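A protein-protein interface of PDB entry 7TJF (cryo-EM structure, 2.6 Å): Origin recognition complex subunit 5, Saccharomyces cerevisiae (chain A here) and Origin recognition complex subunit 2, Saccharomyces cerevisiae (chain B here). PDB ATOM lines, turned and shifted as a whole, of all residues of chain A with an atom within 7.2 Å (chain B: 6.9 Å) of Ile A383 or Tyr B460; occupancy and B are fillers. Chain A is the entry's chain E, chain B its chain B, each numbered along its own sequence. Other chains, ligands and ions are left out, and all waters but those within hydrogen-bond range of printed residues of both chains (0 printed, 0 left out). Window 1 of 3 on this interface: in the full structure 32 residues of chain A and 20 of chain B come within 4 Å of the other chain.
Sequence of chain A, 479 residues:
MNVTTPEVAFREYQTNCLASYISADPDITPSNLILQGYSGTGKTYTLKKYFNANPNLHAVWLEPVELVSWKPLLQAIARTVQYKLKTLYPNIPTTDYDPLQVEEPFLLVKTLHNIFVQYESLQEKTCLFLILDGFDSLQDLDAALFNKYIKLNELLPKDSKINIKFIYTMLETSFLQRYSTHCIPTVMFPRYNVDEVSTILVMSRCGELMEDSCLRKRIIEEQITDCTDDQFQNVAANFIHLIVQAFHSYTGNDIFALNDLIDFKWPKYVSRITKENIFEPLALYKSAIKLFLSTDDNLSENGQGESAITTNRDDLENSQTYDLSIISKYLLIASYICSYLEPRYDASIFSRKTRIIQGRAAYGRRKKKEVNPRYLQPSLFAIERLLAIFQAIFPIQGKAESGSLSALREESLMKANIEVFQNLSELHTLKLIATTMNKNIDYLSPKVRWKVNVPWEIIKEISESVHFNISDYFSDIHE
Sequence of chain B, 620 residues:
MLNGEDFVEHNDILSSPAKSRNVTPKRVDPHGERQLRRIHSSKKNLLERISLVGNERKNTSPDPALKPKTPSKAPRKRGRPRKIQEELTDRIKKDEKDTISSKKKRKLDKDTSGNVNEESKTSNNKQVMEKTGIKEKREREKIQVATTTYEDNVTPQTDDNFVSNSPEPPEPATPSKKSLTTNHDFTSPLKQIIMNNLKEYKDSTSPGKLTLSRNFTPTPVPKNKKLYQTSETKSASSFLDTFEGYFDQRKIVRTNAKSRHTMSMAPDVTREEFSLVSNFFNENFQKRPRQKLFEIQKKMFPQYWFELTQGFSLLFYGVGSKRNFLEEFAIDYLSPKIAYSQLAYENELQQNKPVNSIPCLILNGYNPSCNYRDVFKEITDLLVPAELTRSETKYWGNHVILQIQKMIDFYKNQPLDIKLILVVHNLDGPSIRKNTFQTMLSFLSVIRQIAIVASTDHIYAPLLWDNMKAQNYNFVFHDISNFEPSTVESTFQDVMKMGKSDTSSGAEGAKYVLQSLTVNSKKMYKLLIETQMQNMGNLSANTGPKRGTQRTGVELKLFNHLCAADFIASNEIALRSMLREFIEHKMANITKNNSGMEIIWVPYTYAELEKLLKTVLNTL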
ATOM      1  N   CYS A 338      15.783 -25.525  20.408  1.00  0.00           N
ATOM      2  CA  CYS A 338      17.017 -25.101  19.753  1.00  0.00           C
ATOM      3  C   CYS A 338      17.761 -24.046  20.560  1.00  0.00           C
ATOM      4  O   CYS A 338      18.996 -24.018  20.553  1.00  0.00           O
ATOM      5  CB  CYS A 338      16.712 -24.551  18.361  1.00  0.00           C
ATOM      6  SG  CYS A 338      16.176 -25.739  17.142  1.00  0.00           S
ATOM      7  N   PHE A 381      20.536 -20.068  16.682  1.00  0.00           N
ATOM      8  CA  PHE A 381      20.488 -21.239  15.818  1.00  0.00           C
ATOM      9  C   PHE A 381      20.212 -20.812  14.382  1.00  0.00           C
ATOM     10  O   PHE A 381      19.857 -19.664  14.104  1.00  0.00           O
ATOM     11  CB  PHE A 381      19.430 -22.257  16.286  1.00  0.00           C
ATOM     12  CG  PHE A 381      18.066 -21.663  16.538  1.00  0.00           C
ATOM     13  CD1 PHE A 381      17.124 -21.584  15.517  1.00  0.00           C
ATOM     14  CD2 PHE A 381      17.714 -21.210  17.803  1.00  0.00           C
ATOM     15  CE1 PHE A 381      15.874 -21.047  15.748  1.00  0.00           C
ATOM     16  CE2 PHE A 381      16.464 -20.681  18.040  1.00  0.00           C
ATOM     17  CZ  PHE A 381      15.544 -20.591  17.012  1.00  0.00           C
ATOM     18  N   ALA A 382      20.376 -21.763  13.467  1.00  0.00           N
ATOM     19  CA  ALA A 382      20.044 -21.570  12.065  1.00  0.00           C
ATOM     20  C   ALA A 382      18.615 -22.034  11.784  1.00  0.00           C
ATOM     21  O   ALA A 382      17.959 -22.657  12.620  1.00  0.00           O
ATOM     22  CB  ALA A 382      21.036 -22.313  11.172  1.00  0.00           C
ATOM     23  N   ILE A 383      18.139 -21.712  10.578  1.00  0.00           N
ATOM     24  CA  ILE A 383      16.778 -22.056  10.167  1.00  0.00           C
ATOM     25  C   ILE A 383      16.612 -23.568  10.038  1.00  0.00           C
ATOM     26  O   ILE A 383      15.615 -24.139  10.504  1.00  0.00           O
ATOM     27  CB  ILE A 383      16.433 -21.323   8.854  1.00  0.00           C
ATOM     28  CG1 ILE A 383      16.089 -19.861   9.133  1.00  0.00           C
ATOM     29  CG2 ILE A 383      15.282 -21.991   8.108  1.00  0.00           C
ATOM     30  CD1 ILE A 383      14.822 -19.682   9.941  1.00  0.00           C
ATOM     31  N   GLU A 384      17.595 -24.240   9.433  1.00  0.00           N
ATOM     32  CA  GLU A 384      17.449 -25.657   9.118  1.00  0.00           C
ATOM     33  C   GLU A 384      17.496 -26.538  10.362  1.00  0.00           C
ATOM     34  O   GLU A 384      16.852 -27.589  10.385  1.00  0.00           O
ATOM     35  CB  GLU A 384      18.507 -26.077   8.099  1.00  0.00           C
ATOM     36  CG  GLU A 384      18.176 -27.372   7.364  1.00  0.00           C
ATOM     37  CD  GLU A 384      17.604 -27.143   5.976  1.00  0.00           C
ATOM     38  OE1 GLU A 384      17.883 -26.090   5.375  1.00  0.00           O
ATOM     39  OE2 GLU A 384      16.882 -28.032   5.480  1.00  0.00           O
ATOM     40  N   ARG A 385      18.219 -26.120  11.407  1.00  0.00           N
ATOM     41  CA  ARG A 385      18.165 -26.839  12.679  1.00  0.00           C
ATOM     42  C   ARG A 385      16.779 -26.750  13.309  1.00  0.00           C
ATOM     43  O   ARG A 385      16.254 -27.752  13.822  1.00  0.00           O
ATOM     44  CB  ARG A 385      19.219 -26.291  13.641  1.00  0.00           C
ATOM     45  CG  ARG A 385      19.537 -27.234  14.780  1.00  0.00           C
ATOM     46  CD  ARG A 385      20.243 -26.534  15.917  1.00  0.00           C
ATOM     47  NE  ARG A 385      19.951 -27.177  17.191  1.00  0.00           N
ATOM     48  CZ  ARG A 385      20.151 -26.622  18.377  1.00  0.00           C
ATOM     49  NH1 ARG A 385      20.664 -25.408  18.494  1.00  0.00           N
ATOM     50  NH2 ARG A 385      19.822 -27.298  19.474  1.00  0.00           N
ATOM     51  N   LEU A 386      16.171 -25.556  13.269  1.00  0.00           N
ATOM     52  CA  LEU A 386      14.817 -25.367  13.782  1.00  0.00           C
ATOM     53  C   LEU A 386      13.810 -26.196  13.001  1.00  0.00           C
ATOM     54  O   LEU A 386      12.927 -26.828  13.590  1.00  0.00           O
ATOM     55  CB  LEU A 386      14.439 -23.885  13.740  1.00  0.00           C
ATOM     56  CG  LEU A 386      12.948 -23.528  13.751  1.00  0.00           C
ATOM     57  CD1 LEU A 386      12.335 -23.732  15.124  1.00  0.00           C
ATOM     58  CD2 LEU A 386      12.739 -22.105  13.294  1.00  0.00           C
ATOM     59  N   LEU A 387      13.957 -26.237  11.676  1.00  0.00           N
ATOM     60  CA  LEU A 387      13.038 -27.015  10.855  1.00  0.00           C
ATOM     61  C   LEU A 387      13.240 -28.516  11.050  1.00  0.00           C
ATOM     62  O   LEU A 387      12.269 -29.278  11.027  1.00  0.00           O
ATOM     63  CB  LEU A 387      13.198 -26.625   9.389  1.00  0.00           C
ATOM     64  CG  LEU A 387      12.763 -25.224   8.970  1.00  0.00           C
ATOM     65  CD1 LEU A 387      13.090 -25.001   7.509  1.00  0.00           C
ATOM     66  CD2 LEU A 387      11.279 -25.032   9.227  1.00  0.00           C
ATOM     67  N   ALA A 388      14.483 -28.950  11.277  1.00  0.00           N
ATOM     68  CA  ALA A 388      14.764 -30.360  11.541  1.00  0.00           C
ATOM     69  C   ALA A 388      14.145 -30.818  12.858  1.00  0.00           C
ATOM     70  O   ALA A 388      13.502 -31.874  12.922  1.00  0.00           O
ATOM     71  CB  ALA A 388      16.275 -30.593  11.545  1.00  0.00           C
ATOM     72  N   ILE A 389      14.313 -30.024  13.918  1.00  0.00           N
ATOM     73  CA  ILE A 389      13.722 -30.383  15.205  1.00  0.00           C
ATOM     74  C   ILE A 389      12.196 -30.259  15.172  1.00  0.00           C
ATOM     75  O   ILE A 389      11.487 -31.089  15.766  1.00  0.00           O
ATOM     76  CB  ILE A 389      14.402 -29.552  16.314  1.00  0.00           C
ATOM     77  CG1 ILE A 389      15.740 -30.210  16.661  1.00  0.00           C
ATOM     78  CG2 ILE A 389      13.536 -29.400  17.561  1.00  0.00           C
ATOM     79  CD1 ILE A 389      16.769 -29.290  17.217  1.00  0.00           C
ATOM     80  N   ALA A 416       8.706 -28.740   5.389  1.00  0.00           N
ATOM     81  CA  ALA A 416       8.512 -27.304   5.559  1.00  0.00           C
ATOM     82  C   ALA A 416       8.027 -26.714   4.242  1.00  0.00           C
ATOM     83  O   ALA A 416       8.823 -26.354   3.372  1.00  0.00           O
ATOM     84  CB  ALA A 416       9.805 -26.643   6.018  1.00  0.00           C
ATOM     85  N   PHE A 421       6.885 -21.690   6.657  1.00  0.00           N
ATOM     86  CA  PHE A 421       7.669 -20.464   6.563  1.00  0.00           C
ATOM     87  C   PHE A 421       6.824 -19.227   6.837  1.00  0.00           C
ATOM     88  O   PHE A 421       7.315 -18.271   7.446  1.00  0.00           O
ATOM     89  CB  PHE A 421       8.332 -20.374   5.189  1.00  0.00           C
ATOM     90  CG  PHE A 421       9.538 -21.252   5.049  1.00  0.00           C
ATOM     91  CD1 PHE A 421       9.409 -22.566   4.627  1.00  0.00           C
ATOM     92  CD2 PHE A 421      10.798 -20.774   5.366  1.00  0.00           C
ATOM     93  CE1 PHE A 421      10.518 -23.383   4.509  1.00  0.00           C
ATOM     94  CE2 PHE A 421      11.912 -21.584   5.250  1.00  0.00           C
ATOM     95  CZ  PHE A 421      11.771 -22.891   4.821  1.00  0.00           C
ATOM     96  N   LEU A 424       6.421 -19.115  10.555  1.00  0.00           N
ATOM     97  CA  LEU A 424       7.678 -18.661  11.142  1.00  0.00           C
ATOM     98  C   LEU A 424       7.859 -17.151  10.987  1.00  0.00           C
ATOM     99  O   LEU A 424       8.311 -16.473  11.918  1.00  0.00           O
ATOM    100  CB  LEU A 424       8.837 -19.415  10.493  1.00  0.00           C
ATOM    101  CG  LEU A 424      10.256 -19.239  11.029  1.00  0.00           C
ATOM    102  CD1 LEU A 424      10.286 -19.259  12.554  1.00  0.00           C
ATOM    103  CD2 LEU A 424      11.145 -20.322  10.455  1.00  0.00           C
ATOM    104  N   TYR A 443      16.739 -11.509   5.820  1.00  0.00           N
ATOM    105  CA  TYR A 443      16.178 -12.789   6.244  1.00  0.00           C
ATOM    106  C   TYR A 443      16.869 -13.966   5.569  1.00  0.00           C
ATOM    107  O   TYR A 443      16.971 -15.046   6.162  1.00  0.00           O
ATOM    108  CB  TYR A 443      14.684 -12.838   5.935  1.00  0.00           C
ATOM    109  CG  TYR A 443      13.836 -11.967   6.824  1.00  0.00           C
ATOM    110  CD1 TYR A 443      13.375 -12.426   8.053  1.00  0.00           C
ATOM    111  CD2 TYR A 443      13.486 -10.683   6.428  1.00  0.00           C
ATOM    112  CE1 TYR A 443      12.591 -11.620   8.866  1.00  0.00           C
ATOM    113  CE2 TYR A 443      12.711  -9.875   7.225  1.00  0.00           C
ATOM    114  CZ  TYR A 443      12.264 -10.346   8.442  1.00  0.00           C
ATOM    115  OH  TYR A 443      11.487  -9.530   9.230  1.00  0.00           O
ATOM    116  N   LEU A 444      17.351 -13.780   4.346  1.00  0.00           N
ATOM    117  CA  LEU A 444      17.888 -14.877   3.554  1.00  0.00           C
ATOM    118  C   LEU A 444      19.394 -15.038   3.705  1.00  0.00           C
ATOM    119  O   LEU A 444      19.970 -15.939   3.088  1.00  0.00           O
ATOM    120  CB  LEU A 444      17.531 -14.683   2.076  1.00  0.00           C
ATOM    121  CG  LEU A 444      16.084 -14.278   1.782  1.00  0.00           C
ATOM    122  CD1 LEU A 444      15.856 -14.123   0.291  1.00  0.00           C
ATOM    123  CD2 LEU A 444      15.104 -15.279   2.365  1.00  0.00           C
ATOM    124  N   SER A 445      20.039 -14.193   4.489  1.00  0.00           N
ATOM    125  CA  SER A 445      21.467 -14.353   4.713  1.00  0.00           C
ATOM    126  C   SER A 445      21.724 -15.490   5.700  1.00  0.00           C
ATOM    127  O   SER A 445      20.990 -15.642   6.680  1.00  0.00           O
ATOM    128  CB  SER A 445      22.075 -13.060   5.245  1.00  0.00           C
ATOM    129  OG  SER A 445      23.407 -13.265   5.676  1.00  0.00           O
ATOM    130  N   VAL A 448      22.595 -14.333   9.470  1.00  0.00           N
ATOM    131  CA  VAL A 448      21.540 -13.959  10.403  1.00  0.00           C
ATOM    132  C   VAL A 448      21.027 -15.214  11.097  1.00  0.00           C
ATOM    133  O   VAL A 448      20.571 -16.158  10.445  1.00  0.00           O
ATOM    134  CB  VAL A 448      20.410 -13.215   9.682  1.00  0.00           C
ATOM    135  CG1 VAL A 448      19.200 -13.069  10.585  1.00  0.00           C
ATOM    136  CG2 VAL A 448      20.906 -11.847   9.238  1.00  0.00           C
ATOM    137  N   ARG A 449      21.115 -15.230  12.421  1.00  0.00           N
ATOM    138  CA  ARG A 449      20.660 -16.351  13.226  1.00  0.00           C
ATOM    139  C   ARG A 449      19.433 -15.950  14.036  1.00  0.00           C
ATOM    140  O   ARG A 449      19.073 -14.775  14.135  1.00  0.00           O
ATOM    141  CB  ARG A 449      21.784 -16.855  14.137  1.00  0.00           C
ATOM    142  CG  ARG A 449      22.794 -17.726  13.409  1.00  0.00           C
ATOM    143  CD  ARG A 449      24.013 -18.019  14.258  1.00  0.00           C
ATOM    144  NE  ARG A 449      24.712 -16.803  14.656  1.00  0.00           N
ATOM    145  CZ  ARG A 449      25.318 -16.638  15.823  1.00  0.00           C
ATOM    146  NH1 ARG A 449      25.331 -17.596  16.736  1.00  0.00           N
ATOM    147  NH2 ARG A 449      25.927 -15.484  16.081  1.00  0.00           N
ATOM    148  N   TRP A 450      18.795 -16.962  14.617  1.00  0.00           N
ATOM    149  CA  TRP A 450      17.496 -16.844  15.261  1.00  0.00           C
ATOM    150  C   TRP A 450      17.569 -17.350  16.693  1.00  0.00           C
ATOM    151  O   TRP A 450      18.387 -18.211  17.020  1.00  0.00           O
ATOM    152  CB  TRP A 450      16.433 -17.628  14.473  1.00  0.00           C
ATOM    153  CG  TRP A 450      16.349 -17.219  13.036  1.00  0.00           C
ATOM    154  CD1 TRP A 450      17.136 -17.648  12.007  1.00  0.00           C
ATOM    155  CD2 TRP A 450      15.370 -16.355  12.454  1.00  0.00           C
ATOM    156  NE1 TRP A 450      16.745 -17.055  10.835  1.00  0.00           N
ATOM    157  CE2 TRP A 450      15.650 -16.271  11.078  1.00  0.00           C
ATOM    158  CE3 TRP A 450      14.287 -15.634  12.968  1.00  0.00           C
ATOM    159  CZ2 TRP A 450      14.893 -15.491  10.206  1.00  0.00           C
ATOM    160  CZ3 TRP A 450      13.539 -14.859  12.104  1.00  0.00           C
ATOM    161  CH2 TRP A 450      13.845 -14.793  10.737  1.00  0.00           C
ATOM    162  N   TYR B 246      20.177 -34.758   8.563  1.00  0.00           N
ATOM    163  CA  TYR B 246      20.728 -33.519   9.110  1.00  0.00           C
ATOM    164  C   TYR B 246      21.557 -33.782  10.365  1.00  0.00           C
ATOM    165  O   TYR B 246      22.667 -33.256  10.509  1.00  0.00           O
ATOM    166  CB  TYR B 246      19.597 -32.532   9.409  1.00  0.00           C
ATOM    167  CG  TYR B 246      20.061 -31.202   9.960  1.00  0.00           C
ATOM    168  CD1 TYR B 246      20.522 -30.208   9.113  1.00  0.00           C
ATOM    169  CD2 TYR B 246      20.021 -30.934  11.327  1.00  0.00           C
ATOM    170  CE1 TYR B 246      20.944 -28.987   9.604  1.00  0.00           C
ATOM    171  CE2 TYR B 246      20.444 -29.718  11.830  1.00  0.00           C
ATOM    172  CZ  TYR B 246      20.898 -28.746  10.963  1.00  0.00           C
ATOM    173  OH  TYR B 246      21.322 -27.537  11.452  1.00  0.00           O
ATOM    174  N   ASP B 428      13.343 -12.071  -4.538  1.00  0.00           N
ATOM    175  CA  ASP B 428      14.171 -12.300  -3.365  1.00  0.00           C
ATOM    176  C   ASP B 428      15.606 -11.818  -3.561  1.00  0.00           C
ATOM    177  O   ASP B 428      16.517 -12.324  -2.902  1.00  0.00           O
ATOM    178  CB  ASP B 428      14.152 -13.784  -3.012  1.00  0.00           C
ATOM    179  CG  ASP B 428      14.368 -14.665  -4.223  1.00  0.00           C
ATOM    180  OD1 ASP B 428      14.490 -14.123  -5.342  1.00  0.00           O
ATOM    181  OD2 ASP B 428      14.397 -15.899  -4.065  1.00  0.00           O
ATOM    182  N   ASP B 457      14.514 -16.887  -6.590  1.00  0.00           N
ATOM    183  CA  ASP B 457      15.622 -17.815  -6.751  1.00  0.00           C
ATOM    184  C   ASP B 457      16.099 -18.458  -5.458  1.00  0.00           C
ATOM    185  O   ASP B 457      16.659 -19.558  -5.515  1.00  0.00           O
ATOM    186  CB  ASP B 457      16.820 -17.113  -7.410  1.00  0.00           C
ATOM    187  CG  ASP B 457      16.860 -17.314  -8.905  1.00  0.00           C
ATOM    188  OD1 ASP B 457      16.242 -18.283  -9.390  1.00  0.00           O
ATOM    189  OD2 ASP B 457      17.511 -16.504  -9.597  1.00  0.00           O
ATOM    190  N   HIS B 458      15.908 -17.820  -4.308  1.00  0.00           N
ATOM    191  CA  HIS B 458      16.417 -18.365  -3.059  1.00  0.00           C
ATOM    192  C   HIS B 458      15.528 -19.492  -2.552  1.00  0.00           C
ATOM    193  O   HIS B 458      14.306 -19.478  -2.722  1.00  0.00           O
ATOM    194  CB  HIS B 458      16.529 -17.274  -1.994  1.00  0.00           C
ATOM    195  CG  HIS B 458      17.603 -17.526  -0.985  1.00  0.00           C
ATOM    196  ND1 HIS B 458      17.386 -18.251   0.167  1.00  0.00           N
ATOM    197  CD2 HIS B 458      18.902 -17.148  -0.951  1.00  0.00           C
ATOM    198  CE1 HIS B 458      18.505 -18.312   0.864  1.00  0.00           C
ATOM    199  NE2 HIS B 458      19.441 -17.651   0.208  1.00  0.00           N
ATOM    200  N   ILE B 459      16.163 -20.473  -1.909  1.00  0.00           N
ATOM    201  CA  ILE B 459      15.436 -21.614  -1.367  1.00  0.00           C
ATOM    202  C   ILE B 459      14.620 -21.232  -0.131  1.00  0.00           C
ATOM    203  O   ILE B 459      13.682 -21.950   0.234  1.00  0.00           O
ATOM    204  CB  ILE B 459      16.433 -22.760  -1.084  1.00  0.00           C
ATOM    205  CG1 ILE B 459      15.725 -24.116  -1.070  1.00  0.00           C
ATOM    206  CG2 ILE B 459      17.209 -22.529   0.211  1.00  0.00           C
ATOM    207  CD1 ILE B 459      16.488 -25.206  -1.755  1.00  0.00           C
ATOM    208  N   TYR B 460      14.924 -20.099   0.504  1.00  0.00           N
ATOM    209  CA  TYR B 460      14.232 -19.667   1.711  1.00  0.00           C
ATOM    210  C   TYR B 460      13.331 -18.462   1.473  1.00  0.00           C
ATOM    211  O   TYR B 460      12.979 -17.771   2.430  1.00  0.00           O
ATOM    212  CB  TYR B 460      15.239 -19.349   2.817  1.00  0.00           C
ATOM    213  CG  TYR B 460      15.769 -20.558   3.549  1.00  0.00           C
ATOM    214  CD1 TYR B 460      15.075 -21.764   3.543  1.00  0.00           C
ATOM    215  CD2 TYR B 460      16.963 -20.489   4.255  1.00  0.00           C
ATOM    216  CE1 TYR B 460      15.563 -22.870   4.214  1.00  0.00           C
ATOM    217  CE2 TYR B 460      17.457 -21.585   4.930  1.00  0.00           C
ATOM    218  CZ  TYR B 460      16.755 -22.772   4.906  1.00  0.00           C
ATOM    219  OH  TYR B 460      17.251 -23.861   5.581  1.00  0.00           O
ATOM    220  N   ALA B 461      12.971 -18.190   0.217  1.00  0.00           N
ATOM    221  CA  ALA B 461      12.127 -17.043  -0.125  1.00  0.00           C
ATOM    222  C   ALA B 461      10.765 -16.953   0.585  1.00  0.00           C
ATOM    223  O   ALA B 461      10.385 -15.827   0.950  1.00  0.00           O
ATOM    224  CB  ALA B 461      11.948 -16.986  -1.652  1.00  0.00           C
ATOM    225  N   PRO B 462       9.997 -18.035   0.833  1.00  0.00           N
ATOM    226  CA  PRO B 462       8.744 -17.870   1.602  1.00  0.00           C
ATOM    227  C   PRO B 462       8.915 -17.428   3.055  1.00  0.00           C
ATOM    228  O   PRO B 462       7.907 -17.109   3.699  1.00  0.00           O
ATOM    229  CB  PRO B 462       8.101 -19.259   1.528  1.00  0.00           C
ATOM    230  CG  PRO B 462       8.591 -19.810   0.284  1.00  0.00           C
ATOM    231  CD  PRO B 462      10.014 -19.384   0.224  1.00  0.00           C
ATOM    232  N   LEU B 463      10.139 -17.384   3.587  1.00  0.00           N
ATOM    233  CA  LEU B 463      10.379 -16.765   4.885  1.00  0.00           C
ATOM    234  C   LEU B 463      10.196 -15.250   4.852  1.00  0.00           C
ATOM    235  O   LEU B 463      10.041 -14.635   5.911  1.00  0.00           O
ATOM    236  CB  LEU B 463      11.789 -17.125   5.363  1.00  0.00           C
ATOM    237  CG  LEU B 463      12.281 -16.853   6.781  1.00  0.00           C
ATOM    238  CD1 LEU B 463      11.603 -17.778   7.761  1.00  0.00           C
ATOM    239  CD2 LEU B 463      13.790 -17.011   6.835  1.00  0.00           C
ATOM    240  N   LEU B 464      10.186 -14.637   3.663  1.00  0.00           N
ATOM    241  CA  LEU B 464      10.060 -13.188   3.571  1.00  0.00           C
ATOM    242  C   LEU B 464       8.655 -12.685   3.889  1.00  0.00           C
ATOM    243  O   LEU B 464       8.494 -11.497   4.186  1.00  0.00           O
ATOM    244  CB  LEU B 464      10.464 -12.713   2.173  1.00  0.00           C
ATOM    245  CG  LEU B 464      11.920 -12.933   1.760  1.00  0.00           C
ATOM    246  CD1 LEU B 464      12.117 -12.619   0.284  1.00  0.00           C
ATOM    247  CD2 LEU B 464      12.860 -12.104   2.620  1.00  0.00           C
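Hydrophobic or aromatic side chains of chain A that line the printed part of chain B: Ile A383, Ala A388, Phe A421, Leu A424, Tyr A443, Leu A444 and Trp A450.
Of the 10 printed residues of chain B, 7 touch a printed residue of chain A.
Of chain B, only Tyr B460 (3.6 Å) comes within 4 Å of Ile A383.
Of the printed residues of chain B, Glu A384 touches Tyr B246 (3.9 Å) and Tyr B460 (2.3 Å).
Of the printed residues of chain B, Tyr A443 touches Leu B463 and Leu B464.
Of the printed residues of chain B, Leu A444 touches Asp B428, His B458, Tyr B460 and Leu B464.
Of the printed residues of chain A, Leu B463 touches Phe A421 (3.8 Å), Leu A424 (3.7 Å), Tyr A443 (3.8 Å) and Trp A450 (3.9 Å).
Of the printed residues of chain A, Leu B464 touches Tyr A443 (3.9 Å) and Leu A444 (3.9 Å).
The nearest residue of chain B that does not touch Ile A383 is Leu B463 (4.2 Å).
The nearest residue of chain A that does not touch Tyr B460 is Leu A387 (4.6 Å).
The nearest printed residue of chain A that does not touch Asp B428 is Ser A445 (8.4 Å).
OD2 of Asp B428 lies within hydrogen-bond range of N of Asp B457, 2.7 Å away.
The side-chain carboxylate (OD2) of Asp B428 sits at hydrogen-bond distance from the backbone NH (N) of His B458 (2.5 Å).
The backbone NH (N) of Tyr B460 sits at hydrogen-bond distance from a ring nitrogen (ND1) of His B458, at 3.1 Å.
The guanidinium group (NH1) of Arg A385 sits at hydrogen-bond distance from the backbone carbonyl oxygen (O) of Cys A338, at 3.0 Å.
The backbone NH of Phe A381 is in hydrogen-bond range of the backbone carbonyl oxygen of Trp A450 (2.9 Å).
Ile A383 touches Tyr B460 (CG2 to CZ, 3.6 Å).
CE1 of Tyr B246 touches CG of Glu A384, 3.9 Å away.
Ala A388 touches Tyr B246.
Phe A421 touches Tyr B460 (CE2 to CD1, 3.6 Å).
Phe A421 touches Pro B462 (CB to O, 3.6 Å).
Phe A421 touches Leu B463.
CD2 of Leu B463 touches O of Tyr A443, 3.8 Å away.
Tyr B460 touches Leu A444 (O to CD2, 3.3 Å).
Leu B464 touches Leu A444 (CD2 to CD2, 3.9 Å).
Leu B463 touches Trp A450 (CD2 to CZ2, 3.9 Å).
The side-chain hydroxyl (OH) of Tyr B246 lies close to the backbone NH (N) of Arg A385 (3.4 Å).
The backbone carbonyl oxygen of Leu A444 lies within hydrogen-bond range of a ring nitrogen (NE2) of His B458, at 3.4 Å.
The side-chain carboxylate of Glu A384 sits close to the side-chain hydroxyl of Tyr B460.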
